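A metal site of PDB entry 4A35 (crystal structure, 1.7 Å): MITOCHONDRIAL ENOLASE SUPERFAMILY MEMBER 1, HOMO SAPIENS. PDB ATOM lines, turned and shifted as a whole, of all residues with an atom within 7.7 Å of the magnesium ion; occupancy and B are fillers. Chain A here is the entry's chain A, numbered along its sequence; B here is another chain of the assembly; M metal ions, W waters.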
ATOM      1  N   ASP A  27     -31.164 -15.307  11.698  1.00  0.00           N
ATOM      2  CA  ASP A  27     -30.003 -14.453  11.432  1.00  0.00           C
ATOM      3  C   ASP A  27     -30.549 -13.114  10.915  1.00  0.00           C
ATOM      4  O   ASP A  27     -31.783 -12.929  10.882  1.00  0.00           O
ATOM      5  CB  ASP A  27     -28.960 -15.130  10.503  1.00  0.00           C
ATOM      6  CG  ASP A  27     -29.421 -15.426   9.089  1.00  0.00           C
ATOM      7  OD1 ASP A  27     -29.865 -14.471   8.393  1.00  0.00           O
ATOM      8  OD2 ASP A  27     -29.221 -16.536   8.654  1.00  0.00           O
ATOM      9  N   TYR A 191     -16.062 -25.252  15.759  1.00  0.00           N
ATOM     10  CA  TYR A 191     -16.530 -24.078  16.487  1.00  0.00           C
ATOM     11  C   TYR A 191     -18.013 -24.244  16.599  1.00  0.00           C
ATOM     12  O   TYR A 191     -18.623 -24.954  15.759  1.00  0.00           O
ATOM     13  CB  TYR A 191     -16.151 -22.759  15.776  1.00  0.00           C
ATOM     14  CG  TYR A 191     -16.858 -22.452  14.476  1.00  0.00           C
ATOM     15  CD1 TYR A 191     -18.038 -21.704  14.458  1.00  0.00           C
ATOM     16  CD2 TYR A 191     -16.242 -22.709  13.248  1.00  0.00           C
ATOM     17  CE1 TYR A 191     -18.654 -21.344  13.259  1.00  0.00           C
ATOM     18  CE2 TYR A 191     -16.807 -22.270  12.029  1.00  0.00           C
ATOM     19  CZ  TYR A 191     -18.015 -21.588  12.051  1.00  0.00           C
ATOM     20  OH  TYR A 191     -18.604 -21.197  10.888  1.00  0.00           O
ATOM     21  N   THR A 193     -21.937 -22.546  16.672  1.00  0.00           N
ATOM     22  CA  THR A 193     -22.818 -21.451  16.226  1.00  0.00           C
ATOM     23  C   THR A 193     -24.054 -21.432  17.177  1.00  0.00           C
ATOM     24  O   THR A 193     -24.980 -20.656  16.975  1.00  0.00           O
ATOM     25  CB  THR A 193     -23.113 -21.614  14.727  1.00  0.00           C
ATOM     26  OG1 THR A 193     -21.849 -21.500  14.082  1.00  0.00           O
ATOM     27  CG2 THR A 193     -24.051 -20.483  14.134  1.00  0.00           C
ATOM     28  N   TRP A 197     -27.390 -16.863  17.434  1.00  0.00           N
ATOM     29  CA  TRP A 197     -28.673 -16.449  16.850  1.00  0.00           C
ATOM     30  C   TRP A 197     -29.250 -15.168  17.402  1.00  0.00           C
ATOM     31  O   TRP A 197     -28.953 -14.762  18.535  1.00  0.00           O
ATOM     32  CB  TRP A 197     -29.698 -17.608  16.888  1.00  0.00           C
ATOM     33  CG  TRP A 197     -29.105 -18.932  16.438  1.00  0.00           C
ATOM     34  CD1 TRP A 197     -28.858 -20.029  17.214  1.00  0.00           C
ATOM     35  CD2 TRP A 197     -28.650 -19.263  15.108  1.00  0.00           C
ATOM     36  NE1 TRP A 197     -28.331 -21.059  16.431  1.00  0.00           N
ATOM     37  CE2 TRP A 197     -28.172 -20.597  15.147  1.00  0.00           C
ATOM     38  CE3 TRP A 197     -28.642 -18.574  13.869  1.00  0.00           C
ATOM     39  CZ2 TRP A 197     -27.652 -21.248  14.002  1.00  0.00           C
ATOM     40  CZ3 TRP A 197     -28.222 -19.249  12.730  1.00  0.00           C
ATOM     41  CH2 TRP A 197     -27.695 -20.554  12.810  1.00  0.00           C
ATOM     42  N   LYS A 221     -19.252 -18.506  17.061  1.00  0.00           N
ATOM     43  CA  LYS A 221     -19.726 -17.602  16.032  1.00  0.00           C
ATOM     44  C   LYS A 221     -20.884 -16.806  16.585  1.00  0.00           C
ATOM     45  O   LYS A 221     -21.630 -17.283  17.450  1.00  0.00           O
ATOM     46  CB  LYS A 221     -20.124 -18.328  14.714  1.00  0.00           C
ATOM     47  CG  LYS A 221     -20.325 -17.350  13.554  1.00  0.00           C
ATOM     48  CD  LYS A 221     -19.902 -17.911  12.192  1.00  0.00           C
ATOM     49  CE  LYS A 221     -21.065 -18.668  11.659  1.00  0.00           C
ATOM     50  NZ  LYS A 221     -20.709 -19.390  10.402  1.00  0.00           N
ATOM     51  N   LYS A 223     -24.057 -14.044  15.008  1.00  0.00           N
ATOM     52  CA  LYS A 223     -24.709 -13.383  13.882  1.00  0.00           C
ATOM     53  C   LYS A 223     -24.808 -11.898  14.163  1.00  0.00           C
ATOM     54  O   LYS A 223     -25.161 -11.482  15.289  1.00  0.00           O
ATOM     55  CB  LYS A 223     -26.138 -13.933  13.653  1.00  0.00           C
ATOM     56  CG  LYS A 223     -26.214 -15.415  13.330  1.00  0.00           C
ATOM     57  CD  LYS A 223     -25.456 -15.752  12.020  1.00  0.00           C
ATOM     58  CE  LYS A 223     -25.242 -17.248  11.976  1.00  0.00           C
ATOM     59  NZ  LYS A 223     -25.119 -17.747  10.579  1.00  0.00           N
ATOM     60  N   MET A 250     -17.714 -13.499  13.416  1.00  0.00           N
ATOM     61  CA  MET A 250     -18.987 -12.785  13.108  1.00  0.00           C
ATOM     62  C   MET A 250     -19.522 -13.201  11.740  1.00  0.00           C
ATOM     63  O   MET A 250     -18.726 -13.469  10.809  1.00  0.00           O
ATOM     64  CB  MET A 250     -18.773 -11.269  13.192  1.00  0.00           C
ATOM     65  CG  MET A 250     -18.443 -10.811  14.625  1.00  0.00           C
ATOM     66  SD  MET A 250     -17.962  -9.085  14.547  1.00  0.00           S
ATOM     67  CE  MET A 250     -17.514  -8.735  16.284  1.00  0.00           C
ATOM     68  N   ASP A 251     -20.859 -13.141  11.574  1.00  0.00           N
ATOM     69  CA  ASP A 251     -21.497 -13.577  10.333  1.00  0.00           C
ATOM     70  C   ASP A 251     -22.637 -12.618  10.016  1.00  0.00           C
ATOM     71  O   ASP A 251     -23.580 -12.501  10.796  1.00  0.00           O
ATOM     72  CB  ASP A 251     -21.998 -15.038  10.500  1.00  0.00           C
ATOM     73  CG  ASP A 251     -22.580 -15.640   9.224  1.00  0.00           C
ATOM     74  OD1 ASP A 251     -22.757 -14.885   8.236  1.00  0.00           O
ATOM     75  OD2 ASP A 251     -22.912 -16.848   9.225  1.00  0.00           O
ATOM     76  N   ALA A 252     -22.498 -11.852   8.931  1.00  0.00           N
ATOM     77  CA  ALA A 252     -23.486 -10.835   8.530  1.00  0.00           C
ATOM     78  C   ALA A 252     -24.518 -11.397   7.552  1.00  0.00           C
ATOM     79  O   ALA A 252     -25.415 -10.626   7.201  1.00  0.00           O
ATOM     80  CB  ALA A 252     -22.791  -9.628   7.910  1.00  0.00           C
ATOM     81  N   ASN A 253     -24.373 -12.676   7.087  1.00  0.00           N
ATOM     82  CA  ASN A 253     -25.374 -13.270   6.145  1.00  0.00           C
ATOM     83  C   ASN A 253     -25.796 -12.299   5.006  1.00  0.00           C
ATOM     84  O   ASN A 253     -27.020 -12.159   4.687  1.00  0.00           O
ATOM     85  CB  ASN A 253     -26.653 -13.705   6.940  1.00  0.00           C
ATOM     86  CG  ASN A 253     -26.366 -14.907   7.813  1.00  0.00           C
ATOM     87  OD1 ASN A 253     -26.060 -14.757   8.992  1.00  0.00           O
ATOM     88  ND2 ASN A 253     -26.251 -16.087   7.204  1.00  0.00           N
ATOM     89  N   GLN A 254     -24.757 -11.660   4.357  1.00  0.00           N
ATOM     90  CA  GLN A 254     -24.921 -10.867   3.118  1.00  0.00           C
ATOM     91  C   GLN A 254     -25.656  -9.542   3.302  1.00  0.00           C
ATOM     92  O   GLN A 254     -26.066  -8.947   2.321  1.00  0.00           O
ATOM     93  CB  GLN A 254     -25.692 -11.695   2.023  1.00  0.00           C
ATOM     94  CG  GLN A 254     -25.200 -13.146   1.902  1.00  0.00           C
ATOM     95  CD  GLN A 254     -26.200 -14.075   1.220  1.00  0.00           C
ATOM     96  OE1 GLN A 254     -27.330 -13.690   0.891  1.00  0.00           O
ATOM     97  NE2 GLN A 254     -25.823 -15.344   1.056  1.00  0.00           N
ATOM     98  N   TRP A 275     -12.840 -13.417  11.946  1.00  0.00           N
ATOM     99  CA  TRP A 275     -13.324 -13.153  10.619  1.00  0.00           C
ATOM    100  C   TRP A 275     -14.721 -12.535  10.646  1.00  0.00           C
ATOM    101  O   TRP A 275     -15.470 -12.641  11.662  1.00  0.00           O
ATOM    102  CB  TRP A 275     -13.346 -14.424   9.735  1.00  0.00           C
ATOM    103  CG  TRP A 275     -14.386 -15.491  10.011  1.00  0.00           C
ATOM    104  CD1 TRP A 275     -15.738 -15.372   9.890  1.00  0.00           C
ATOM    105  CD2 TRP A 275     -14.116 -16.891  10.156  1.00  0.00           C
ATOM    106  NE1 TRP A 275     -16.341 -16.603  10.091  1.00  0.00           N
ATOM    107  CE2 TRP A 275     -15.374 -17.559  10.236  1.00  0.00           C
ATOM    108  CE3 TRP A 275     -12.915 -17.655  10.261  1.00  0.00           C
ATOM    109  CZ2 TRP A 275     -15.476 -18.956  10.368  1.00  0.00           C
ATOM    110  CZ3 TRP A 275     -13.022 -19.029  10.422  1.00  0.00           C
ATOM    111  CH2 TRP A 275     -14.285 -19.670  10.447  1.00  0.00           C
ATOM    112  N   GLU A 277     -17.931 -13.025   8.238  1.00  0.00           N
ATOM    113  CA  GLU A 277     -18.434 -13.960   7.247  1.00  0.00           C
ATOM    114  C   GLU A 277     -19.590 -13.297   6.441  1.00  0.00           C
ATOM    115  O   GLU A 277     -20.467 -12.640   7.009  1.00  0.00           O
ATOM    116  CB  GLU A 277     -18.886 -15.230   7.970  1.00  0.00           C
ATOM    117  CG  GLU A 277     -19.543 -16.280   7.077  1.00  0.00           C
ATOM    118  CD  GLU A 277     -19.831 -17.548   7.889  1.00  0.00           C
ATOM    119  OE1 GLU A 277     -19.088 -17.775   8.872  1.00  0.00           O
ATOM    120  OE2 GLU A 277     -20.685 -18.372   7.473  1.00  0.00           O
ATOM    121  N   GLU A 278     -19.616 -13.562   5.101  1.00  0.00           N
ATOM    122  CA  GLU A 278     -20.596 -13.055   4.159  1.00  0.00           C
ATOM    123  C   GLU A 278     -20.928 -11.563   4.414  1.00  0.00           C
ATOM    124  O   GLU A 278     -22.104 -11.219   4.644  1.00  0.00           O
ATOM    125  CB  GLU A 278     -21.873 -13.897   4.188  1.00  0.00           C
ATOM    126  CG  GLU A 278     -21.669 -15.292   3.629  1.00  0.00           C
ATOM    127  CD  GLU A 278     -22.975 -15.775   3.057  1.00  0.00           C
ATOM    128  OE1 GLU A 278     -23.914 -16.045   3.863  1.00  0.00           O
ATOM    129  OE2 GLU A 278     -23.084 -15.881   1.810  1.00  0.00           O
ATOM    130  N   ALA A 303     -14.420 -14.106   5.401  1.00  0.00           N
ATOM    131  CA  ALA A 303     -14.848 -15.494   5.142  1.00  0.00           C
ATOM    132  C   ALA A 303     -16.101 -15.473   4.243  1.00  0.00           C
ATOM    133  O   ALA A 303     -17.002 -14.668   4.475  1.00  0.00           O
ATOM    134  CB  ALA A 303     -15.184 -16.220   6.462  1.00  0.00           C
ATOM    135  N   THR A 304     -16.182 -16.369   3.266  1.00  0.00           N
ATOM    136  CA  THR A 304     -17.435 -16.458   2.515  1.00  0.00           C
ATOM    137  C   THR A 304     -17.486 -17.807   1.840  1.00  0.00           C
ATOM    138  O   THR A 304     -16.461 -18.510   1.781  1.00  0.00           O
ATOM    139  CB  THR A 304     -17.652 -15.262   1.493  1.00  0.00           C
ATOM    140  OG1 THR A 304     -19.006 -15.361   0.969  1.00  0.00           O
ATOM    141  CG2 THR A 304     -16.653 -15.319   0.298  1.00  0.00           C
ATOM    142  N   GLY A 305     -18.674 -18.144   1.339  1.00  0.00           N
ATOM    143  CA  GLY A 305     -18.814 -19.351   0.547  1.00  0.00           C
ATOM    144  C   GLY A 305     -20.035 -20.210   0.730  1.00  0.00           C
ATOM    145  O   GLY A 305     -20.335 -20.992  -0.178  1.00  0.00           O
ATOM    146  N   GLU A 306     -20.711 -20.154   1.898  1.00  0.00           N
ATOM    147  CA  GLU A 306     -21.842 -21.069   2.093  1.00  0.00           C
ATOM    148  C   GLU A 306     -22.940 -20.965   0.998  1.00  0.00           C
ATOM    149  O   GLU A 306     -23.576 -21.981   0.758  1.00  0.00           O
ATOM    150  CB  GLU A 306     -22.506 -20.856   3.459  1.00  0.00           C
ATOM    151  CG  GLU A 306     -23.361 -19.613   3.539  1.00  0.00           C
ATOM    152  CD  GLU A 306     -23.861 -19.412   4.946  1.00  0.00           C
ATOM    153  OE1 GLU A 306     -23.008 -19.407   5.857  1.00  0.00           O
ATOM    154  OE2 GLU A 306     -25.088 -19.320   5.142  1.00  0.00           O
ATOM    155  N   GLN A 307     -23.168 -19.758   0.339  1.00  0.00           N
ATOM    156  CA  GLN A 307     -24.174 -19.637  -0.709  1.00  0.00           C
ATOM    157  C   GLN A 307     -23.498 -19.415  -2.058  1.00  0.00           C
ATOM    158  O   GLN A 307     -24.185 -19.094  -3.036  1.00  0.00           O
ATOM    159  CB  GLN A 307     -25.184 -18.494  -0.385  1.00  0.00           C
ATOM    160  CG  GLN A 307     -26.127 -18.876   0.775  1.00  0.00           C
ATOM    161  CD  GLN A 307     -27.541 -18.334   0.609  1.00  0.00           C
ATOM    162  OE1 GLN A 307     -28.017 -17.510   1.411  1.00  0.00           O
ATOM    163  NE2 GLN A 307     -28.297 -18.888  -0.327  1.00  0.00           N
ATOM    164  N   GLN A 327     -15.295 -20.973   2.670  1.00  0.00           N
ATOM    165  CA  GLN A 327     -16.279 -21.840   3.308  1.00  0.00           C
ATOM    166  C   GLN A 327     -17.029 -22.695   2.296  1.00  0.00           C
ATOM    167  O   GLN A 327     -18.036 -22.264   1.757  1.00  0.00           O
ATOM    168  CB  GLN A 327     -17.243 -20.977   4.147  1.00  0.00           C
ATOM    169  CG  GLN A 327     -16.367 -20.173   5.155  1.00  0.00           C
ATOM    170  CD  GLN A 327     -17.102 -19.159   5.920  1.00  0.00           C
ATOM    171  OE1 GLN A 327     -17.732 -18.271   5.334  1.00  0.00           O
ATOM    172  NE2 GLN A 327     -17.002 -19.265   7.241  1.00  0.00           N
ATOM    173  N   HIS A 356     -18.846 -24.615   6.000  1.00  0.00           N
ATOM    174  CA  HIS A 356     -20.123 -24.221   6.530  1.00  0.00           C
ATOM    175  C   HIS A 356     -20.849 -25.517   6.935  1.00  0.00           C
ATOM    176  O   HIS A 356     -20.738 -26.552   6.266  1.00  0.00           O
ATOM    177  CB  HIS A 356     -20.951 -23.410   5.495  1.00  0.00           C
ATOM    178  CG  HIS A 356     -22.410 -23.256   5.822  1.00  0.00           C
ATOM    179  ND1 HIS A 356     -23.395 -24.016   5.168  1.00  0.00           N
ATOM    180  CD2 HIS A 356     -23.014 -22.435   6.697  1.00  0.00           C
ATOM    181  CE1 HIS A 356     -24.555 -23.613   5.672  1.00  0.00           C
ATOM    182  NE2 HIS A 356     -24.391 -22.654   6.583  1.00  0.00           N
ATOM    183  N   ALA A 357     -21.650 -25.429   7.972  1.00  0.00           N
ATOM    184  CA  ALA A 357     -22.437 -26.591   8.381  1.00  0.00           C
ATOM    185  C   ALA A 357     -23.702 -26.131   9.166  1.00  0.00           C
ATOM    186  O   ALA A 357     -24.164 -24.993   8.953  1.00  0.00           O
ATOM    187  CB  ALA A 357     -21.567 -27.558   9.183  1.00  0.00           C
ATOM    188  N   GLU A 387     -17.479 -25.700  11.063  1.00  0.00           N
ATOM    189  CA  GLU A 387     -18.625 -25.225  11.834  1.00  0.00           C
ATOM    190  C   GLU A 387     -19.402 -26.403  12.462  1.00  0.00           C
ATOM    191  O   GLU A 387     -19.484 -27.487  11.879  1.00  0.00           O
ATOM    192  CB  GLU A 387     -19.554 -24.409  10.945  1.00  0.00           C
ATOM    193  CG  GLU A 387     -20.770 -23.793  11.638  1.00  0.00           C
ATOM    194  CD  GLU A 387     -21.481 -22.748  10.789  1.00  0.00           C
ATOM    195  OE1 GLU A 387     -21.476 -22.874   9.539  1.00  0.00           O
ATOM    196  OE2 GLU A 387     -22.065 -21.806  11.385  1.00  0.00           O
ATOM    197  N   TRP B 104     -33.196 -18.566  -0.158  1.00  0.00           N
ATOM    198  CA  TRP B 104     -32.165 -19.604   0.011  1.00  0.00           C
ATOM    199  C   TRP B 104     -32.023 -20.434  -1.270  1.00  0.00           C
ATOM    200  O   TRP B 104     -30.931 -20.927  -1.559  1.00  0.00           O
ATOM    201  CB  TRP B 104     -32.544 -20.559   1.160  1.00  0.00           C
ATOM    202  CG  TRP B 104     -31.417 -21.474   1.570  1.00  0.00           C
ATOM    203  CD1 TRP B 104     -31.242 -22.779   1.187  1.00  0.00           C
ATOM    204  CD2 TRP B 104     -30.331 -21.159   2.435  1.00  0.00           C
ATOM    205  NE1 TRP B 104     -30.092 -23.278   1.744  1.00  0.00           N
ATOM    206  CE2 TRP B 104     -29.528 -22.328   2.553  1.00  0.00           C
ATOM    207  CE3 TRP B 104     -29.950 -19.997   3.140  1.00  0.00           C
ATOM    208  CZ2 TRP B 104     -28.319 -22.331   3.264  1.00  0.00           C
ATOM    209  CZ3 TRP B 104     -28.787 -20.029   3.908  1.00  0.00           C
ATOM    210  CH2 TRP B 104     -28.013 -21.197   3.991  1.00  0.00           C
HETATM  211 MG    MG M   1     -22.852 -18.210   7.537  1.00  0.00          MG
HETATM  212  O   HOH W   1     -25.231 -18.595   7.705  1.00  0.00           O
HETATM  213  O   HOH W   2     -23.218 -16.651   6.430  1.00  0.00           O
HETATM  214  O   HOH W   3     -23.122 -19.765   8.695  1.00  0.00           O
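OD2 of Asp 251 sits close to NZ of Lys 221 (3.6 Å).
The indole nitrogen of Trp 275 is in hydrogen-bond range of the side-chain carboxylate of Glu 277.
The side-chain amino group (NZ) of Lys 221 is in salt-bridge range of the side-chain carboxylate (OE2) of Glu 387.
NZ of Lys 221 lies within salt-bridge range of OE1 of Glu 277, 2.8 Å away.
The backbone NH of Glu 277 lies within hydrogen-bond range of the backbone carbonyl oxygen of Met 250, 2.7 Å away.
The backbone carbonyl oxygen (O) of Glu 277 lies within hydrogen-bond range of the backbone NH (N) of Ala 252 (2.9 Å).
The backbone NH of Glu 306 sits at hydrogen-bond distance from the backbone carbonyl oxygen of Gln 327 (3.4 Å).
The side-chain amide nitrogen (NE2) of Gln 327 is in hydrogen-bond range of the side-chain carboxylate (OE1) of Glu 277 (3.0 Å).
Lys 221 touches the magnesium ion.
NZ of Lys 223 touches the magnesium ion, 3.8 Å away.
Five residues have an atom within 4 Å of the magnesium ion: Lys 221, Lys 223, Asp 251, Glu 277 and Glu 306.
The nearest printed residue that does not touch the magnesium ion is Asn 253 (4.02 Å).
The magnesium ion is bound by water W2 (1.9 Å), water W3 (2.0 Å), the side-chain carboxylate of Glu 306 (2.1 Å), the side-chain carboxylate of Asp 251 (2.2 Å), the side-chain carboxylate of Glu 277 (2.2 Å) and water W1 (2.4 Å).
Water W1 lies within hydrogen-bond range of the side-chain carboxylate (OE2) of Glu 306, the side-chain amide nitrogen (ND2) of Asn 253 and the side-chain amino group (NZ) of Lys 223.
Water W3 bridges the side-chain amino group (NZ) of Lys 221 (3.0 Å) and the side-chain amino group (NZ) of Lys 223 (3.4 Å).
Water W2 lies within hydrogen-bond range of OD1 of Asp 251 (2.6 Å), OE1 of Glu 278 (2.7 Å) and ND2 of Asn 253 (3.2 Å).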
